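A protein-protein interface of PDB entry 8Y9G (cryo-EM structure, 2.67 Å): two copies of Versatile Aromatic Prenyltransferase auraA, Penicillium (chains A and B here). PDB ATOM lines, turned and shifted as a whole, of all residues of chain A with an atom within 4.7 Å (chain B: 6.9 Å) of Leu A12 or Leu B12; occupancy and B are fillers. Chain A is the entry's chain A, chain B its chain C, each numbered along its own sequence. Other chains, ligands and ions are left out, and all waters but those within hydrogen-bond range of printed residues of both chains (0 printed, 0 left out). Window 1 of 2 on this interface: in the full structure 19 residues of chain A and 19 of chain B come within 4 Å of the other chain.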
ATOM      1  N   LEU A   8      10.287  27.505 -13.963  1.00  0.00           N
ATOM      2  CA  LEU A   8       9.242  26.554 -14.313  1.00  0.00           C
ATOM      3  C   LEU A   8       7.871  27.212 -14.331  1.00  0.00           C
ATOM      4  O   LEU A   8       7.113  27.048 -15.290  1.00  0.00           O
ATOM      5  CB  LEU A   8       9.269  25.384 -13.337  1.00  0.00           C
ATOM      6  CG  LEU A   8      10.302  24.298 -13.608  1.00  0.00           C
ATOM      7  CD1 LEU A   8      10.235  23.233 -12.554  1.00  0.00           C
ATOM      8  CD2 LEU A   8      10.101  23.693 -14.969  1.00  0.00           C
ATOM      9  N   GLY A   9       7.531  27.961 -13.283  1.00  0.00           N
ATOM     10  CA  GLY A   9       6.267  28.674 -13.286  1.00  0.00           C
ATOM     11  C   GLY A   9       6.169  29.663 -14.427  1.00  0.00           C
ATOM     12  O   GLY A   9       5.072  29.985 -14.892  1.00  0.00           O
ATOM     13  N   ARG A  10       7.314  30.157 -14.895  1.00  0.00           N
ATOM     14  CA  ARG A  10       7.304  31.060 -16.040  1.00  0.00           C
ATOM     15  C   ARG A  10       7.010  30.308 -17.335  1.00  0.00           C
ATOM     16  O   ARG A  10       6.314  30.826 -18.216  1.00  0.00           O
ATOM     17  CB  ARG A  10       8.636  31.802 -16.128  1.00  0.00           C
ATOM     18  CG  ARG A  10       8.852  32.793 -15.004  1.00  0.00           C
ATOM     19  CD  ARG A  10       9.685  33.967 -15.431  1.00  0.00           C
ATOM     20  NE  ARG A  10      11.049  33.587 -15.781  1.00  0.00           N
ATOM     21  CZ  ARG A  10      12.102  33.735 -14.984  1.00  0.00           C
ATOM     22  NH1 ARG A  10      11.968  34.241 -13.768  1.00  0.00           N
ATOM     23  NH2 ARG A  10      13.301  33.364 -15.404  1.00  0.00           N
ATOM     24  N   VAL A  11       7.520  29.081 -17.468  1.00  0.00           N
ATOM     25  CA  VAL A  11       7.368  28.355 -18.728  1.00  0.00           C
ATOM     26  C   VAL A  11       6.156  27.429 -18.704  1.00  0.00           C
ATOM     27  O   VAL A  11       5.453  27.290 -19.710  1.00  0.00           O
ATOM     28  CB  VAL A  11       8.651  27.571 -19.065  1.00  0.00           C
ATOM     29  CG1 VAL A  11       9.798  28.505 -19.315  1.00  0.00           C
ATOM     30  CG2 VAL A  11       8.994  26.594 -17.982  1.00  0.00           C
ATOM     31  N   LEU A  12       5.891  26.778 -17.576  1.00  0.00           N
ATOM     32  CA  LEU A  12       4.968  25.651 -17.570  1.00  0.00           C
ATOM     33  C   LEU A  12       3.547  26.081 -17.908  1.00  0.00           C
ATOM     34  O   LEU A  12       3.068  27.126 -17.460  1.00  0.00           O
ATOM     35  CB  LEU A  12       4.987  24.954 -16.213  1.00  0.00           C
ATOM     36  CG  LEU A  12       6.253  24.185 -15.846  1.00  0.00           C
ATOM     37  CD1 LEU A  12       6.124  23.611 -14.455  1.00  0.00           C
ATOM     38  CD2 LEU A  12       6.541  23.111 -16.860  1.00  0.00           C
ATOM     39  N   GLN A  13       2.872  25.215 -18.585  1.00  0.00           N
ATOM     40  CA  GLN A  13       1.513  25.387 -18.889  1.00  0.00           C
ATOM     41  C   GLN A  13       0.738  24.584 -17.923  1.00  0.00           C
ATOM     42  O   GLN A  13       1.099  23.479 -17.693  1.00  0.00           O
ATOM     43  CB  GLN A  13       1.217  24.860 -20.295  1.00  0.00           C
ATOM     44  CG  GLN A  13       1.880  25.503 -21.491  1.00  0.00           C
ATOM     45  CD  GLN A  13       1.690  26.986 -21.558  1.00  0.00           C
ATOM     46  OE1 GLN A  13       2.652  27.744 -21.536  1.00  0.00           O
ATOM     47  NE2 GLN A  13       0.451  27.413 -21.658  1.00  0.00           N
ATOM     48  N   PHE A  14      -0.368  25.076 -17.400  1.00  0.00           N
ATOM     49  CA  PHE A  14      -1.102  24.431 -16.372  1.00  0.00           C
ATOM     50  C   PHE A  14      -2.399  24.132 -16.830  1.00  0.00           C
ATOM     51  O   PHE A  14      -2.970  24.984 -17.361  1.00  0.00           O
ATOM     52  CB  PHE A  14      -1.136  25.296 -15.129  1.00  0.00           C
ATOM     53  CG  PHE A  14       0.173  25.432 -14.416  1.00  0.00           C
ATOM     54  CD1 PHE A  14       1.013  26.458 -14.705  1.00  0.00           C
ATOM     55  CD2 PHE A  14       0.525  24.575 -13.420  1.00  0.00           C
ATOM     56  CE1 PHE A  14       2.202  26.621 -14.043  1.00  0.00           C
ATOM     57  CE2 PHE A  14       1.701  24.737 -12.743  1.00  0.00           C
ATOM     58  CZ  PHE A  14       2.552  25.758 -13.064  1.00  0.00           C
ATOM     59  N   TRP A  23       0.822  25.671  -7.330  1.00  0.00           N
ATOM     60  CA  TRP A  23       2.227  25.800  -7.678  1.00  0.00           C
ATOM     61  C   TRP A  23       2.833  27.026  -7.016  1.00  0.00           C
ATOM     62  O   TRP A  23       3.830  26.924  -6.295  1.00  0.00           O
ATOM     63  CB  TRP A  23       2.379  25.878  -9.194  1.00  0.00           C
ATOM     64  CG  TRP A  23       3.792  26.047  -9.628  1.00  0.00           C
ATOM     65  CD1 TRP A  23       4.445  27.219  -9.840  1.00  0.00           C
ATOM     66  CD2 TRP A  23       4.738  25.010  -9.888  1.00  0.00           C
ATOM     67  NE1 TRP A  23       5.733  26.979 -10.217  1.00  0.00           N
ATOM     68  CE2 TRP A  23       5.941  25.628 -10.256  1.00  0.00           C
ATOM     69  CE3 TRP A  23       4.683  23.616  -9.848  1.00  0.00           C
ATOM     70  CZ2 TRP A  23       7.075  24.908 -10.581  1.00  0.00           C
ATOM     71  CZ3 TRP A  23       5.809  22.908 -10.171  1.00  0.00           C
ATOM     72  CH2 TRP A  23       6.990  23.552 -10.534  1.00  0.00           C
ATOM     73  N   LEU A  49       8.664  18.899 -11.524  1.00  0.00           N
ATOM     74  CA  LEU A  49       7.838  18.480 -12.650  1.00  0.00           C
ATOM     75  C   LEU A  49       6.926  17.325 -12.261  1.00  0.00           C
ATOM     76  O   LEU A  49       5.801  17.218 -12.760  1.00  0.00           O
ATOM     77  CB  LEU A  49       8.730  18.100 -13.826  1.00  0.00           C
ATOM     78  CG  LEU A  49       9.485  19.263 -14.464  1.00  0.00           C
ATOM     79  CD1 LEU A  49      10.739  18.789 -15.171  1.00  0.00           C
ATOM     80  CD2 LEU A  49       8.586  20.002 -15.412  1.00  0.00           C
ATOM     81  N   TYR A  52       4.087  18.892 -10.466  1.00  0.00           N
ATOM     82  CA  TYR A  52       3.273  19.510 -11.436  1.00  0.00           C
ATOM     83  C   TYR A  52       2.409  18.559 -12.196  1.00  0.00           C
ATOM     84  O   TYR A  52       1.297  18.879 -12.511  1.00  0.00           O
ATOM     85  CB  TYR A  52       4.258  20.223 -12.363  1.00  0.00           C
ATOM     86  CG  TYR A  52       3.826  20.531 -13.766  1.00  0.00           C
ATOM     87  CD1 TYR A  52       2.988  21.590 -14.037  1.00  0.00           C
ATOM     88  CD2 TYR A  52       4.297  19.795 -14.825  1.00  0.00           C
ATOM     89  CE1 TYR A  52       2.584  21.865 -15.310  1.00  0.00           C
ATOM     90  CE2 TYR A  52       3.897  20.073 -16.093  1.00  0.00           C
ATOM     91  CZ  TYR A  52       3.046  21.105 -16.309  1.00  0.00           C
ATOM     92  OH  TYR A  52       2.690  21.380 -17.560  1.00  0.00           O
ATOM     93  N   PRO B   4      16.624  14.323 -20.187  1.00  0.00           N
ATOM     94  CA  PRO B   4      15.690  15.434 -19.951  1.00  0.00           C
ATOM     95  C   PRO B   4      14.529  15.502 -20.927  1.00  0.00           C
ATOM     96  O   PRO B   4      13.414  15.843 -20.520  1.00  0.00           O
ATOM     97  CB  PRO B   4      16.599  16.662 -20.056  1.00  0.00           C
ATOM     98  CG  PRO B   4      17.920  16.178 -19.640  1.00  0.00           C
ATOM     99  CD  PRO B   4      18.027  14.758 -20.084  1.00  0.00           C
ATOM    100  N   TRP B   5      14.749  15.181 -22.202  1.00  0.00           N
ATOM    101  CA  TRP B   5      13.672  15.302 -23.179  1.00  0.00           C
ATOM    102  C   TRP B   5      12.638  14.195 -23.013  1.00  0.00           C
ATOM    103  O   TRP B   5      11.436  14.442 -23.149  1.00  0.00           O
ATOM    104  CB  TRP B   5      14.238  15.324 -24.602  1.00  0.00           C
ATOM    105  CG  TRP B   5      15.303  14.314 -24.912  1.00  0.00           C
ATOM    106  CD1 TRP B   5      15.145  13.151 -25.599  1.00  0.00           C
ATOM    107  CD2 TRP B   5      16.690  14.392 -24.575  1.00  0.00           C
ATOM    108  NE1 TRP B   5      16.338  12.495 -25.699  1.00  0.00           N
ATOM    109  CE2 TRP B   5      17.305  13.236 -25.078  1.00  0.00           C
ATOM    110  CE3 TRP B   5      17.470  15.323 -23.887  1.00  0.00           C
ATOM    111  CZ2 TRP B   5      18.660  12.983 -24.914  1.00  0.00           C
ATOM    112  CZ3 TRP B   5      18.812  15.069 -23.726  1.00  0.00           C
ATOM    113  CH2 TRP B   5      19.395  13.910 -24.237  1.00  0.00           C
ATOM    114  N   PHE B   7      11.798  12.641 -20.079  1.00  0.00           N
ATOM    115  CA  PHE B   7      11.006  13.003 -18.911  1.00  0.00           C
ATOM    116  C   PHE B   7      10.116  14.206 -19.201  1.00  0.00           C
ATOM    117  O   PHE B   7       8.936  14.227 -18.827  1.00  0.00           O
ATOM    118  CB  PHE B   7      11.936  13.275 -17.728  1.00  0.00           C
ATOM    119  CG  PHE B   7      11.219  13.695 -16.488  1.00  0.00           C
ATOM    120  CD1 PHE B   7      10.585  12.762 -15.690  1.00  0.00           C
ATOM    121  CD2 PHE B   7      11.177  15.022 -16.117  1.00  0.00           C
ATOM    122  CE1 PHE B   7       9.924  13.151 -14.552  1.00  0.00           C
ATOM    123  CE2 PHE B   7      10.518  15.408 -14.982  1.00  0.00           C
ATOM    124  CZ  PHE B   7       9.890  14.471 -14.199  1.00  0.00           C
ATOM    125  N   LEU B   8      10.664  15.219 -19.870  1.00  0.00           N
ATOM    126  CA  LEU B   8       9.893  16.422 -20.156  1.00  0.00           C
ATOM    127  C   LEU B   8       8.692  16.116 -21.039  1.00  0.00           C
ATOM    128  O   LEU B   8       7.573  16.540 -20.737  1.00  0.00           O
ATOM    129  CB  LEU B   8      10.794  17.464 -20.808  1.00  0.00           C
ATOM    130  CG  LEU B   8      11.667  18.286 -19.869  1.00  0.00           C
ATOM    131  CD1 LEU B   8      12.519  19.244 -20.648  1.00  0.00           C
ATOM    132  CD2 LEU B   8      10.826  19.035 -18.872  1.00  0.00           C
ATOM    133  N   GLY B   9       8.898  15.387 -22.133  1.00  0.00           N
ATOM    134  CA  GLY B   9       7.773  15.002 -22.967  1.00  0.00           C
ATOM    135  C   GLY B   9       6.762  14.166 -22.216  1.00  0.00           C
ATOM    136  O   GLY B   9       5.575  14.159 -22.549  1.00  0.00           O
ATOM    137  N   ARG B  10       7.217  13.451 -21.186  1.00  0.00           N
ATOM    138  CA  ARG B  10       6.290  12.678 -20.370  1.00  0.00           C
ATOM    139  C   ARG B  10       5.454  13.585 -19.470  1.00  0.00           C
ATOM    140  O   ARG B  10       4.265  13.327 -19.249  1.00  0.00           O
ATOM    141  CB  ARG B  10       7.058  11.646 -19.546  1.00  0.00           C
ATOM    142  CG  ARG B  10       7.670  10.542 -20.380  1.00  0.00           C
ATOM    143  CD  ARG B  10       7.752   9.241 -19.633  1.00  0.00           C
ATOM    144  NE  ARG B  10       8.655   9.310 -18.489  1.00  0.00           N
ATOM    145  CZ  ARG B  10       9.899   8.845 -18.482  1.00  0.00           C
ATOM    146  NH1 ARG B  10      10.423   8.285 -19.562  1.00  0.00           N
ATOM    147  NH2 ARG B  10      10.632   8.950 -17.385  1.00  0.00           N
ATOM    148  N   VAL B  11       6.053  14.661 -18.950  1.00  0.00           N
ATOM    149  CA  VAL B  11       5.341  15.505 -17.992  1.00  0.00           C
ATOM    150  C   VAL B  11       4.668  16.691 -18.677  1.00  0.00           C
ATOM    151  O   VAL B  11       3.556  17.080 -18.306  1.00  0.00           O
ATOM    152  CB  VAL B  11       6.287  15.981 -16.873  1.00  0.00           C
ATOM    153  CG1 VAL B  11       6.771  14.823 -16.053  1.00  0.00           C
ATOM    154  CG2 VAL B  11       7.446  16.752 -17.431  1.00  0.00           C
ATOM    155  N   LEU B  12       5.317  17.289 -19.670  1.00  0.00           N
ATOM    156  CA  LEU B  12       4.898  18.601 -20.145  1.00  0.00           C
ATOM    157  C   LEU B  12       3.519  18.555 -20.787  1.00  0.00           C
ATOM    158  O   LEU B  12       3.182  17.624 -21.522  1.00  0.00           O
ATOM    159  CB  LEU B  12       5.915  19.154 -21.139  1.00  0.00           C
ATOM    160  CG  LEU B  12       7.276  19.562 -20.586  1.00  0.00           C
ATOM    161  CD1 LEU B  12       8.172  20.030 -21.710  1.00  0.00           C
ATOM    162  CD2 LEU B  12       7.131  20.616 -19.522  1.00  0.00           C
ATOM    163  N   GLN B  13       2.809  19.615 -20.601  1.00  0.00           N
ATOM    164  CA  GLN B  13       1.559  19.802 -21.211  1.00  0.00           C
ATOM    165  C   GLN B  13       1.759  20.686 -22.375  1.00  0.00           C
ATOM    166  O   GLN B  13       2.435  21.649 -22.239  1.00  0.00           O
ATOM    167  CB  GLN B  13       0.605  20.492 -20.238  1.00  0.00           C
ATOM    168  CG  GLN B  13       0.286  19.814 -18.929  1.00  0.00           C
ATOM    169  CD  GLN B  13      -0.318  18.456 -19.101  1.00  0.00           C
ATOM    170  OE1 GLN B  13       0.215  17.466 -18.614  1.00  0.00           O
ATOM    171  NE2 GLN B  13      -1.437  18.396 -19.784  1.00  0.00           N
ATOM    172  N   PHE B  14       1.130  20.429 -23.506  1.00  0.00           N
ATOM    173  CA  PHE B  14       1.364  21.145 -24.707  1.00  0.00           C
ATOM    174  C   PHE B  14       0.178  21.784 -25.118  1.00  0.00           C
ATOM    175  O   PHE B  14      -0.782  21.144 -25.124  1.00  0.00           O
ATOM    176  CB  PHE B  14       1.891  20.212 -25.777  1.00  0.00           C
ATOM    177  CG  PHE B  14       3.282  19.704 -25.545  1.00  0.00           C
ATOM    178  CD1 PHE B  14       3.487  18.533 -24.889  1.00  0.00           C
ATOM    179  CD2 PHE B  14       4.364  20.362 -26.038  1.00  0.00           C
ATOM    180  CE1 PHE B  14       4.748  18.032 -24.694  1.00  0.00           C
ATOM    181  CE2 PHE B  14       5.623  19.866 -25.861  1.00  0.00           C
ATOM    182  CZ  PHE B  14       5.820  18.700 -25.174  1.00  0.00           C
ATOM    183  N   LYS B  20       3.521  19.218 -29.731  1.00  0.00           N
ATOM    184  CA  LYS B  20       3.924  17.891 -29.281  1.00  0.00           C
ATOM    185  C   LYS B  20       4.694  17.150 -30.366  1.00  0.00           C
ATOM    186  O   LYS B  20       5.709  16.501 -30.087  1.00  0.00           O
ATOM    187  CB  LYS B  20       2.681  17.111 -28.861  1.00  0.00           C
ATOM    188  CG  LYS B  20       2.929  15.713 -28.344  1.00  0.00           C
ATOM    189  CD  LYS B  20       4.116  15.646 -27.416  1.00  0.00           C
ATOM    190  CE  LYS B  20       4.252  14.283 -26.795  1.00  0.00           C
ATOM    191  NZ  LYS B  20       5.627  14.057 -26.317  1.00  0.00           N
ATOM    192  N   TRP B  23       8.058  18.718 -30.730  1.00  0.00           N
ATOM    193  CA  TRP B  23       8.871  18.282 -29.606  1.00  0.00           C
ATOM    194  C   TRP B  23       9.437  16.895 -29.857  1.00  0.00           C
ATOM    195  O   TRP B  23      10.653  16.692 -29.804  1.00  0.00           O
ATOM    196  CB  TRP B  23       8.036  18.298 -28.329  1.00  0.00           C
ATOM    197  CG  TRP B  23       8.790  17.830 -27.136  1.00  0.00           C
ATOM    198  CD1 TRP B  23       8.869  16.559 -26.668  1.00  0.00           C
ATOM    199  CD2 TRP B  23       9.593  18.628 -26.264  1.00  0.00           C
ATOM    200  NE1 TRP B  23       9.664  16.510 -25.560  1.00  0.00           N
ATOM    201  CE2 TRP B  23      10.123  17.770 -25.289  1.00  0.00           C
ATOM    202  CE3 TRP B  23       9.913  19.984 -26.211  1.00  0.00           C
ATOM    203  CZ2 TRP B  23      10.950  18.220 -24.277  1.00  0.00           C
ATOM    204  CZ3 TRP B  23      10.732  20.426 -25.206  1.00  0.00           C
ATOM    205  CH2 TRP B  23      11.242  19.547 -24.252  1.00  0.00           C
ATOM    206  N   LEU B  48      15.525  23.246 -23.112  1.00  0.00           N
ATOM    207  CA  LEU B  48      14.396  22.528 -23.678  1.00  0.00           C
ATOM    208  C   LEU B  48      13.075  23.142 -23.249  1.00  0.00           C
ATOM    209  O   LEU B  48      12.112  23.129 -24.016  1.00  0.00           O
ATOM    210  CB  LEU B  48      14.468  21.061 -23.276  1.00  0.00           C
ATOM    211  CG  LEU B  48      15.587  20.259 -23.933  1.00  0.00           C
ATOM    212  CD1 LEU B  48      15.911  19.033 -23.126  1.00  0.00           C
ATOM    213  CD2 LEU B  48      15.202  19.881 -25.343  1.00  0.00           C
ATOM    214  N   LEU B  49      13.016  23.726 -22.055  1.00  0.00           N
ATOM    215  CA  LEU B  49      11.806  24.425 -21.641  1.00  0.00           C
ATOM    216  C   LEU B  49      11.637  25.729 -22.409  1.00  0.00           C
ATOM    217  O   LEU B  49      10.511  26.146 -22.698  1.00  0.00           O
ATOM    218  CB  LEU B  49      11.848  24.676 -20.138  1.00  0.00           C
ATOM    219  CG  LEU B  49      11.742  23.424 -19.273  1.00  0.00           C
ATOM    220  CD1 LEU B  49      12.366  23.639 -17.908  1.00  0.00           C
ATOM    221  CD2 LEU B  49      10.306  23.006 -19.142  1.00  0.00           C
ATOM    222  N   TYR B  52      10.225  24.746 -25.692  1.00  0.00           N
ATOM    223  CA  TYR B  52       8.868  24.426 -25.480  1.00  0.00           C
ATOM    224  C   TYR B  52       7.983  25.620 -25.334  1.00  0.00           C
ATOM    225  O   TYR B  52       6.877  25.606 -25.797  1.00  0.00           O
ATOM    226  CB  TYR B  52       8.864  23.576 -24.206  1.00  0.00           C
ATOM    227  CG  TYR B  52       7.601  23.508 -23.396  1.00  0.00           C
ATOM    228  CD1 TYR B  52       6.546  22.711 -23.786  1.00  0.00           C
ATOM    229  CD2 TYR B  52       7.482  24.199 -22.214  1.00  0.00           C
ATOM    230  CE1 TYR B  52       5.392  22.656 -23.058  1.00  0.00           C
ATOM    231  CE2 TYR B  52       6.334  24.139 -21.490  1.00  0.00           C
ATOM    232  CZ  TYR B  52       5.309  23.367 -21.927  1.00  0.00           C
ATOM    233  OH  TYR B  52       4.202  23.302 -21.189  1.00  0.00           O
ATOM    234  N   ASP B  53       8.431  26.644 -24.642  1.00  0.00           N
ATOM    235  CA  ASP B  53       7.546  27.767 -24.367  1.00  0.00           C
ATOM    236  C   ASP B  53       7.610  28.854 -25.433  1.00  0.00           C
ATOM    237  O   ASP B  53       6.571  29.367 -25.860  1.00  0.00           O
ATOM    238  CB  ASP B  53       7.891  28.365 -23.004  1.00  0.00           C
ATOM    239  CG  ASP B  53       6.700  29.002 -22.337  1.00  0.00           C
ATOM    240  OD1 ASP B  53       5.695  28.297 -22.102  1.00  0.00           O
ATOM    241  OD2 ASP B  53       6.766  30.214 -22.046  1.00  0.00           O
ATOM    242  N   ARG B 124       8.056  36.395 -25.397  1.00  0.00           N
ATOM    243  CA  ARG B 124       8.229  35.250 -24.513  1.00  0.00           C
ATOM    244  C   ARG B 124       9.667  35.139 -24.037  1.00  0.00           C
ATOM    245  O   ARG B 124       9.917  34.934 -22.847  1.00  0.00           O
ATOM    246  CB  ARG B 124       7.806  33.960 -25.216  1.00  0.00           C
ATOM    247  CG  ARG B 124       6.364  33.906 -25.668  1.00  0.00           C
ATOM    248  CD  ARG B 124       5.387  34.004 -24.516  1.00  0.00           C
ATOM    249  NE  ARG B 124       5.425  32.832 -23.650  1.00  0.00           N
ATOM    250  CZ  ARG B 124       4.911  32.796 -22.425  1.00  0.00           C
ATOM    251  NH1 ARG B 124       4.320  33.869 -21.918  1.00  0.00           N
ATOM    252  NH2 ARG B 124       4.987  31.690 -21.703  1.00  0.00           N
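O of Val A11 sits close to OD1 of Asp B53 (2.6 Å).
OH of Tyr B52 sits close to N of Gln A13, 3.5 Å away.
OE1 of Gln A13 lies close to OD1 of Asp B53 (3.1 Å).
The side-chain hydroxyl of Tyr A52 is in hydrogen-bond range of the backbone carbonyl oxygen of Gln A13, at 2.6 Å.
The backbone carbonyl oxygen (O) of Val A11 lies close to the side-chain amide oxygen (OE1) of Gln A13.
O of Val B11 sits close to OE1 of Gln B13 (3.4 Å).
The side-chain carboxylate (OD2) of Asp B53 is in salt-bridge range of the guanidinium group (NE) of Arg B124 (3.4 Å).
O of Gln B13 is in hydrogen-bond range of OH of Tyr B52 (2.6 Å).
Among the printed residues, merely in contact across the chains: Tyr A52 with Gln B13 (3.2 Å), Leu A49 with Phe B7 (3.4 Å), Leu A12 with Leu B12 (3.7 Å), Leu A49 with Leu B8 (3.7 Å), Leu A8 with Leu B49 (3.7 Å), Val A11 with Tyr B52 (3.7 Å), Tyr A52 with Val B11 (3.7 Å), Arg A10 with Arg B124 (3.8 Å), Arg A10 with Asp B53 (3.9 Å), Gln A13 with Gln B13 (3.9 Å), Leu A49 with Val B11 (3.99 Å) and Val A11 with Leu B49 (3.99 Å).
Of the printed residues of chain B, Arg A10 touches Asp B53 (3.9 Å) and Arg B124 (3.8 Å).
Leu A12 touches just one residue of chain B: Leu B12 (3.7 Å).
Of the printed residues of chain B, Tyr A52 touches Val B11 and Gln B13.
Pro B4 touches none of the printed residues of chain A.
Of the printed residues of chain A, Phe B7 touches Leu A49.
Of the printed residues of chain A, Leu B8 touches Leu A49.
Arg B10 touches none of the printed residues of chain A.
Leu B12 touches just one residue of chain A: Leu A12 (3.7 Å).
Of the printed residues of chain A, Leu B49 touches Leu A8 and Val A11.
Of the 17 printed residues of chain B, 9 touch a printed residue of chain A.
Hydrophobic or aromatic side chains of chain B that line the printed part of chain A: Phe B7, Leu B8, Val B11, Leu B12, Leu B49 and Tyr B52.
Of the 10 printed residues of chain A, 7 touch a printed residue of chain B.
Printed residues of chain A that touch a printed residue of chain B: Leu A8, Arg A10, Val A11, Leu A12, Gln A13, Leu A49 and Tyr A52.
Hydrophobic or aromatic side chains of chain A that line the printed part of chain B: Leu A8, Val A11, Leu A12, Leu A49 and Tyr A52.
Leu A8 touches Leu B49, and with the chains exchanged Leu A49 touches Leu B8.
Val A11 touches Tyr B52, and with the chains exchanged Tyr A52 touches Val B11.
Leu B12 touches its own counterpart, Leu A12.
Gln A13 touches Tyr B52, and with the chains exchanged Tyr A52 touches Gln B13.
10 positions are printed for both chains.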
